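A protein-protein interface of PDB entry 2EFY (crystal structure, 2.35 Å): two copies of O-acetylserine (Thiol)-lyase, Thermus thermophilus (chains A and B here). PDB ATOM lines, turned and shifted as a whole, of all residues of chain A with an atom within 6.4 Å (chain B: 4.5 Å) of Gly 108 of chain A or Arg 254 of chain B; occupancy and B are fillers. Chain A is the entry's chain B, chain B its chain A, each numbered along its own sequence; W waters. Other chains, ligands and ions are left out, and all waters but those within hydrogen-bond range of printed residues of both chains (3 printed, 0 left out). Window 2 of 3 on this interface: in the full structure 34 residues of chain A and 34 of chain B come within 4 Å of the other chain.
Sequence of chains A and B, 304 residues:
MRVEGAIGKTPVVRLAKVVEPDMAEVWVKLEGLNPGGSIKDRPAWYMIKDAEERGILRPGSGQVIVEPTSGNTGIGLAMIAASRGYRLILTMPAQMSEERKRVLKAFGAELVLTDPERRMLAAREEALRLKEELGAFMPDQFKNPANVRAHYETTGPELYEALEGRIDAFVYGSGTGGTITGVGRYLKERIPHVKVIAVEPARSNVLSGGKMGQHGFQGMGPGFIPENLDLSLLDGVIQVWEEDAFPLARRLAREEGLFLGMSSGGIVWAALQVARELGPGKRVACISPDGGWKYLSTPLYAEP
The backbone carbonyl oxygen (O) of Lys 105 of chain A is in hydrogen-bond range of the guanidinium group (NH1) of Arg 254 of chain B (3.1 Å). The backbone carbonyl oxygen (O) of Arg 254 of chain B lies close to the backbone carbonyl oxygen (O) of Ala 82 of chain A (3.3 Å). O of Glu 255 of chain B lies close to O of Ala 82 of chain A (3.1 Å).
OE2 of Glu 255 of chain B is in salt-bridge range of NE of Arg 251 of chain B, 2.6 Å away.
Among the printed residues, pairs that only touch across the chains: Ala 106 of chain A with Ala 253 of chain B (3.2 Å), Gly 108 of chain A with Arg 254 of chain B (3.4 Å), Ala 82 of chain A with Ala 253 of chain B (3.4 Å), Phe 107 of chain A with Ala 253 of chain B (3.5 Å), Ala 106 of chain A with Arg 254 of chain B (3.7 Å), Ser 83 of chain A with Glu 256 of chain B (3.7 Å) and Ser 83 of chain A with Glu 255 of chain B (3.97 Å).
Gly 108 of chain A touches just one residue of chain B: Arg 254 (3.4 Å). Of chain A, only Ala 82 (3.3 Å), Lys 105 (3.1 Å), Ala 106 (3.7 Å) and Gly 108 (3.4 Å) come within 4 Å of Arg 254 of chain B. Of the printed residues of chain A, Glu 255 of chain B touches Ala 82 (3.1 Å) and Ser 83 (3.97 Å). Of the printed residues of chain B, Ala 82 of chain A touches Ala 253 (3.4 Å), Arg 254 (3.3 Å) and Glu 255 (3.1 Å). Of the printed residues of chain A, Glu 256 of chain B touches Ser 83 (3.7 Å). Of the printed residues of chain B, Ala 106 of chain A touches Ala 253 (3.2 Å) and Arg 254 (3.7 Å). Of the printed residues of chain B, Ser 83 of chain A touches Glu 255 and Glu 256. The nearest residue of chain A that does not touch Arg 254 of chain B is Phe 107 of chain A (4.1 Å).
Of the 7 printed residues of chain B, 4 touch a printed residue of chain A. Hydrophobic or aromatic side chains of chain B within 4 Å of the printed part of chain A: Ala 253. Among the printed residues, no Asp or Glu carboxylate lies within 4 Å of a Lys or Arg side-chain nitrogen of the other chain.
No position is printed for both chains.
Water W2 bridges the backbone carbonyl oxygen of Phe 107 of chain A (2.7 Å) and the backbone carbonyl oxygen of Arg 254 of chain B (3.0 Å). Water W1 lies within hydrogen-bond range of the backbone carbonyl oxygen of Ala 82 of chain A (2.8 Å) and the backbone carbonyl oxygen of Arg 254 of chain B (3.1 Å). Water W3 bridges OE2 of Glu 256 of chain B (3.4 Å) and O of Ser 83 of chain A (3.4 Å).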
ATOM      1  N   ALA A  78     -26.105  21.414  20.733  1.00  0.00           N
ATOM      2  CA  ALA A  78     -25.103  22.114  21.527  1.00  0.00           C
ATOM      3  C   ALA A  78     -24.245  22.997  20.624  1.00  0.00           C
ATOM      4  O   ALA A  78     -23.946  24.145  20.953  1.00  0.00           O
ATOM      5  CB  ALA A  78     -24.227  21.110  22.256  1.00  0.00           C
ATOM      6  N   ALA A  81     -26.556  25.855  19.293  1.00  0.00           N
ATOM      7  CA  ALA A  81     -26.894  26.816  20.337  1.00  0.00           C
ATOM      8  C   ALA A  81     -25.680  27.692  20.600  1.00  0.00           C
ATOM      9  O   ALA A  81     -25.808  28.895  20.840  1.00  0.00           O
ATOM     10  CB  ALA A  81     -27.315  26.095  21.621  1.00  0.00           C
ATOM     11  N   ALA A  82     -24.498  27.085  20.551  1.00  0.00           N
ATOM     12  CA  ALA A  82     -23.260  27.830  20.781  1.00  0.00           C
ATOM     13  C   ALA A  82     -23.006  28.826  19.648  1.00  0.00           C
ATOM     14  O   ALA A  82     -22.599  29.964  19.887  1.00  0.00           O
ATOM     15  CB  ALA A  82     -22.088  26.868  20.901  1.00  0.00           C
ATOM     16  N   SER A  83     -23.265  28.396  18.417  1.00  0.00           N
ATOM     17  CA  SER A  83     -23.052  29.245  17.249  1.00  0.00           C
ATOM     18  C   SER A  83     -24.023  30.423  17.170  1.00  0.00           C
ATOM     19  O   SER A  83     -23.646  31.531  16.775  1.00  0.00           O
ATOM     20  CB  SER A  83     -23.182  28.414  15.964  1.00  0.00           C
ATOM     21  OG  SER A  83     -22.958  29.211  14.810  1.00  0.00           O
ATOM     22  N   GLY A  85     -25.827  31.734  19.796  1.00  0.00           N
ATOM     23  CA  GLY A  85     -26.075  32.382  21.069  1.00  0.00           C
ATOM     24  C   GLY A  85     -27.358  32.028  21.798  1.00  0.00           C
ATOM     25  O   GLY A  85     -28.100  32.920  22.212  1.00  0.00           O
ATOM     26  N   TYR A  86     -27.630  30.737  21.962  1.00  0.00           N
ATOM     27  CA  TYR A  86     -28.818  30.298  22.682  1.00  0.00           C
ATOM     28  C   TYR A  86     -28.364  29.501  23.908  1.00  0.00           C
ATOM     29  O   TYR A  86     -27.289  28.898  23.896  1.00  0.00           O
ATOM     30  CB  TYR A  86     -29.696  29.412  21.788  1.00  0.00           C
ATOM     31  CG  TYR A  86     -30.353  30.128  20.627  1.00  0.00           C
ATOM     32  CD1 TYR A  86     -30.306  29.594  19.338  1.00  0.00           C
ATOM     33  CD2 TYR A  86     -31.036  31.332  20.814  1.00  0.00           C
ATOM     34  CE1 TYR A  86     -30.923  30.248  18.260  1.00  0.00           C
ATOM     35  CE2 TYR A  86     -31.654  31.984  19.750  1.00  0.00           C
ATOM     36  CZ  TYR A  86     -31.592  31.437  18.481  1.00  0.00           C
ATOM     37  OH  TYR A  86     -32.205  32.077  17.436  1.00  0.00           O
ATOM     38  N   ARG A  87     -29.176  29.509  24.965  1.00  0.00           N
ATOM     39  CA  ARG A  87     -28.845  28.777  26.183  1.00  0.00           C
ATOM     40  C   ARG A  87     -29.510  27.408  26.136  1.00  0.00           C
ATOM     41  O   ARG A  87     -30.721  27.293  26.339  1.00  0.00           O
ATOM     42  CB  ARG A  87     -29.334  29.533  27.419  1.00  0.00           C
ATOM     43  CG  ARG A  87     -28.921  28.872  28.725  1.00  0.00           C
ATOM     44  CD  ARG A  87     -29.768  29.345  29.897  1.00  0.00           C
ATOM     45  NE  ARG A  87     -29.446  28.634  31.134  1.00  0.00           N
ATOM     46  CZ  ARG A  87     -30.216  28.627  32.222  1.00  0.00           C
ATOM     47  NH1 ARG A  87     -31.364  29.293  32.227  1.00  0.00           N
ATOM     48  NH2 ARG A  87     -29.842  27.954  33.305  1.00  0.00           N
ATOM     49  N   LEU A  88     -28.714  26.377  25.865  1.00  0.00           N
ATOM     50  CA  LEU A  88     -29.224  25.012  25.774  1.00  0.00           C
ATOM     51  C   LEU A  88     -29.126  24.212  27.066  1.00  0.00           C
ATOM     52  O   LEU A  88     -28.135  24.288  27.795  1.00  0.00           O
ATOM     53  CB  LEU A  88     -28.488  24.250  24.668  1.00  0.00           C
ATOM     54  CG  LEU A  88     -28.826  22.763  24.487  1.00  0.00           C
ATOM     55  CD1 LEU A  88     -30.283  22.595  24.087  1.00  0.00           C
ATOM     56  CD2 LEU A  88     -27.915  22.165  23.440  1.00  0.00           C
ATOM     57  N   VAL A 103     -17.785  17.084  26.183  1.00  0.00           N
ATOM     58  CA  VAL A 103     -17.961  17.647  24.856  1.00  0.00           C
ATOM     59  C   VAL A 103     -19.153  18.592  24.877  1.00  0.00           C
ATOM     60  O   VAL A 103     -19.078  19.694  24.333  1.00  0.00           O
ATOM     61  CB  VAL A 103     -18.186  16.541  23.784  1.00  0.00           C
ATOM     62  CG1 VAL A 103     -19.471  15.791  24.059  1.00  0.00           C
ATOM     63  CG2 VAL A 103     -18.226  17.164  22.389  1.00  0.00           C
ATOM     64  N   LEU A 104     -20.242  18.169  25.523  1.00  0.00           N
ATOM     65  CA  LEU A 104     -21.447  18.991  25.604  1.00  0.00           C
ATOM     66  C   LEU A 104     -21.163  20.280  26.365  1.00  0.00           C
ATOM     67  O   LEU A 104     -21.611  21.359  25.965  1.00  0.00           O
ATOM     68  CB  LEU A 104     -22.588  18.223  26.286  1.00  0.00           C
ATOM     69  CG  LEU A 104     -23.131  17.005  25.532  1.00  0.00           C
ATOM     70  CD1 LEU A 104     -24.207  16.319  26.368  1.00  0.00           C
ATOM     71  CD2 LEU A 104     -23.695  17.434  24.181  1.00  0.00           C
ATOM     72  N   LYS A 105     -20.409  20.175  27.452  1.00  0.00           N
ATOM     73  CA  LYS A 105     -20.075  21.358  28.232  1.00  0.00           C
ATOM     74  C   LYS A 105     -19.043  22.218  27.504  1.00  0.00           C
ATOM     75  O   LYS A 105     -18.929  23.416  27.766  1.00  0.00           O
ATOM     76  CB  LYS A 105     -19.546  20.966  29.615  1.00  0.00           C
ATOM     77  CG  LYS A 105     -20.580  20.299  30.521  1.00  0.00           C
ATOM     78  CD  LYS A 105     -19.991  20.023  31.902  1.00  0.00           C
ATOM     79  CE  LYS A 105     -20.985  19.319  32.815  1.00  0.00           C
ATOM     80  NZ  LYS A 105     -20.396  19.049  34.163  1.00  0.00           N
ATOM     81  N   ALA A 106     -18.280  21.615  26.598  1.00  0.00           N
ATOM     82  CA  ALA A 106     -17.295  22.393  25.847  1.00  0.00           C
ATOM     83  C   ALA A 106     -18.066  23.395  24.976  1.00  0.00           C
ATOM     84  O   ALA A 106     -17.606  24.515  24.735  1.00  0.00           O
ATOM     85  CB  ALA A 106     -16.429  21.471  24.983  1.00  0.00           C
ATOM     86  N   PHE A 107     -19.248  22.980  24.517  1.00  0.00           N
ATOM     87  CA  PHE A 107     -20.109  23.832  23.698  1.00  0.00           C
ATOM     88  C   PHE A 107     -20.938  24.756  24.568  1.00  0.00           C
ATOM     89  O   PHE A 107     -21.749  25.528  24.059  1.00  0.00           O
ATOM     90  CB  PHE A 107     -21.054  22.997  22.830  1.00  0.00           C
ATOM     91  CG  PHE A 107     -20.414  22.466  21.594  1.00  0.00           C
ATOM     92  CD1 PHE A 107     -20.259  21.099  21.409  1.00  0.00           C
ATOM     93  CD2 PHE A 107     -19.953  23.334  20.613  1.00  0.00           C
ATOM     94  CE1 PHE A 107     -19.649  20.605  20.260  1.00  0.00           C
ATOM     95  CE2 PHE A 107     -19.343  22.849  19.459  1.00  0.00           C
ATOM     96  CZ  PHE A 107     -19.190  21.482  19.282  1.00  0.00           C
ATOM     97  N   GLY A 108     -20.754  24.653  25.881  1.00  0.00           N
ATOM     98  CA  GLY A 108     -21.472  25.508  26.811  1.00  0.00           C
ATOM     99  C   GLY A 108     -22.865  25.050  27.177  1.00  0.00           C
ATOM    100  O   GLY A 108     -23.632  25.806  27.773  1.00  0.00           O
ATOM    101  N   ALA A 109     -23.207  23.820  26.821  1.00  0.00           N
ATOM    102  CA  ALA A 109     -24.528  23.305  27.144  1.00  0.00           C
ATOM    103  C   ALA A 109     -24.586  22.997  28.631  1.00  0.00           C
ATOM    104  O   ALA A 109     -23.560  22.801  29.279  1.00  0.00           O
ATOM    105  CB  ALA A 109     -24.824  22.044  26.337  1.00  0.00           C
ATOM    106  N   GLU A 110     -25.797  22.957  29.166  1.00  0.00           N
ATOM    107  CA  GLU A 110     -25.999  22.666  30.573  1.00  0.00           C
ATOM    108  C   GLU A 110     -26.647  21.289  30.645  1.00  0.00           C
ATOM    109  O   GLU A 110     -27.536  20.969  29.857  1.00  0.00           O
ATOM    110  CB  GLU A 110     -26.889  23.745  31.187  1.00  0.00           C
ATOM    111  CG  GLU A 110     -27.184  23.574  32.652  1.00  0.00           C
ATOM    112  CD  GLU A 110     -27.949  24.763  33.225  1.00  0.00           C
ATOM    113  OE1 GLU A 110     -28.587  24.597  34.292  1.00  0.00           O
ATOM    114  OE2 GLU A 110     -27.902  25.862  32.615  1.00  0.00           O
ATOM    115  N   ARG B 250     -11.553  27.664  23.970  1.00  0.00           N
ATOM    116  CA  ARG B 250     -12.791  27.543  24.722  1.00  0.00           C
ATOM    117  C   ARG B 250     -13.811  28.553  24.188  1.00  0.00           C
ATOM    118  O   ARG B 250     -14.996  28.232  24.034  1.00  0.00           O
ATOM    119  CB  ARG B 250     -12.533  27.732  26.224  1.00  0.00           C
ATOM    120  CG  ARG B 250     -11.913  26.486  26.887  1.00  0.00           C
ATOM    121  CD  ARG B 250     -11.981  26.531  28.418  1.00  0.00           C
ATOM    122  NE  ARG B 250     -10.829  27.197  29.022  1.00  0.00           N
ATOM    123  CZ  ARG B 250      -9.603  26.676  29.072  1.00  0.00           C
ATOM    124  NH1 ARG B 250      -9.368  25.475  28.555  1.00  0.00           N
ATOM    125  NH2 ARG B 250      -8.609  27.352  29.639  1.00  0.00           N
ATOM    126  N   ARG B 251     -13.358  29.762  23.875  1.00  0.00           N
ATOM    127  CA  ARG B 251     -14.282  30.743  23.327  1.00  0.00           C
ATOM    128  C   ARG B 251     -14.812  30.230  21.977  1.00  0.00           C
ATOM    129  O   ARG B 251     -15.987  30.400  21.661  1.00  0.00           O
ATOM    130  CB  ARG B 251     -13.602  32.099  23.119  1.00  0.00           C
ATOM    131  CG  ARG B 251     -13.349  32.909  24.387  1.00  0.00           C
ATOM    132  CD  ARG B 251     -13.023  34.357  24.013  1.00  0.00           C
ATOM    133  NE  ARG B 251     -14.167  34.978  23.354  1.00  0.00           N
ATOM    134  CZ  ARG B 251     -14.111  36.070  22.598  1.00  0.00           C
ATOM    135  NH1 ARG B 251     -12.954  36.689  22.387  1.00  0.00           N
ATOM    136  NH2 ARG B 251     -15.221  36.539  22.048  1.00  0.00           N
ATOM    137  N   LEU B 252     -13.946  29.588  21.197  1.00  0.00           N
ATOM    138  CA  LEU B 252     -14.341  29.074  19.889  1.00  0.00           C
ATOM    139  C   LEU B 252     -15.442  28.037  19.965  1.00  0.00           C
ATOM    140  O   LEU B 252     -16.370  28.040  19.155  1.00  0.00           O
ATOM    141  CB  LEU B 252     -13.139  28.480  19.167  1.00  0.00           C
ATOM    142  CG  LEU B 252     -12.117  29.529  18.744  1.00  0.00           C
ATOM    143  CD1 LEU B 252     -10.852  28.846  18.189  1.00  0.00           C
ATOM    144  CD2 LEU B 252     -12.760  30.438  17.714  1.00  0.00           C
ATOM    145  N   ALA B 253     -15.334  27.142  20.936  1.00  0.00           N
ATOM    146  CA  ALA B 253     -16.339  26.114  21.094  1.00  0.00           C
ATOM    147  C   ALA B 253     -17.656  26.756  21.531  1.00  0.00           C
ATOM    148  O   ALA B 253     -18.701  26.561  20.906  1.00  0.00           O
ATOM    149  CB  ALA B 253     -15.873  25.093  22.138  1.00  0.00           C
ATOM    150  N   ARG B 254     -17.565  27.536  22.601  1.00  0.00           N
ATOM    151  CA  ARG B 254     -18.693  28.213  23.221  1.00  0.00           C
ATOM    152  C   ARG B 254     -19.400  29.294  22.404  1.00  0.00           C
ATOM    153  O   ARG B 254     -20.624  29.384  22.425  1.00  0.00           O
ATOM    154  CB  ARG B 254     -18.231  28.836  24.538  1.00  0.00           C
ATOM    155  CG  ARG B 254     -19.227  28.723  25.671  1.00  0.00           C
ATOM    156  CD  ARG B 254     -18.822  27.622  26.645  1.00  0.00           C
ATOM    157  NE  ARG B 254     -17.562  27.927  27.324  1.00  0.00           N
ATOM    158  CZ  ARG B 254     -17.032  27.186  28.297  1.00  0.00           C
ATOM    159  NH1 ARG B 254     -17.654  26.089  28.711  1.00  0.00           N
ATOM    160  NH2 ARG B 254     -15.879  27.546  28.859  1.00  0.00           N
ATOM    161  N   GLU B 255     -18.635  30.112  21.687  1.00  0.00           N
ATOM    162  CA  GLU B 255     -19.218  31.219  20.934  1.00  0.00           C
ATOM    163  C   GLU B 255     -19.386  31.030  19.438  1.00  0.00           C
ATOM    164  O   GLU B 255     -20.254  31.658  18.830  1.00  0.00           O
ATOM    165  CB  GLU B 255     -18.393  32.485  21.182  1.00  0.00           C
ATOM    166  CG  GLU B 255     -18.358  32.929  22.639  1.00  0.00           C
ATOM    167  CD  GLU B 255     -17.383  34.058  22.868  1.00  0.00           C
ATOM    168  OE1 GLU B 255     -17.455  35.066  22.138  1.00  0.00           O
ATOM    169  OE2 GLU B 255     -16.537  33.941  23.778  1.00  0.00           O
ATOM    170  N   GLU B 256     -18.561  30.179  18.839  1.00  0.00           N
ATOM    171  CA  GLU B 256     -18.631  29.964  17.398  1.00  0.00           C
ATOM    172  C   GLU B 256     -19.135  28.569  17.074  1.00  0.00           C
ATOM    173  O   GLU B 256     -19.450  28.265  15.926  1.00  0.00           O
ATOM    174  CB  GLU B 256     -17.250  30.158  16.776  1.00  0.00           C
ATOM    175  CG  GLU B 256     -16.535  31.421  17.241  1.00  0.00           C
ATOM    176  CD  GLU B 256     -16.667  32.595  16.272  1.00  0.00           C
ATOM    177  OE1 GLU B 256     -16.030  33.632  16.531  1.00  0.00           O
ATOM    178  OE2 GLU B 256     -17.393  32.490  15.258  1.00  0.00           O
HETATM  179  O   HOH W   1     -23.182  31.201  22.291  1.00  0.00           O
HETATM  180  O   HOH W   2     -22.326  28.112  24.526  1.00  0.00           O
HETATM  181  O   HOH W   3     -20.735  31.937  15.011  1.00  0.00           O
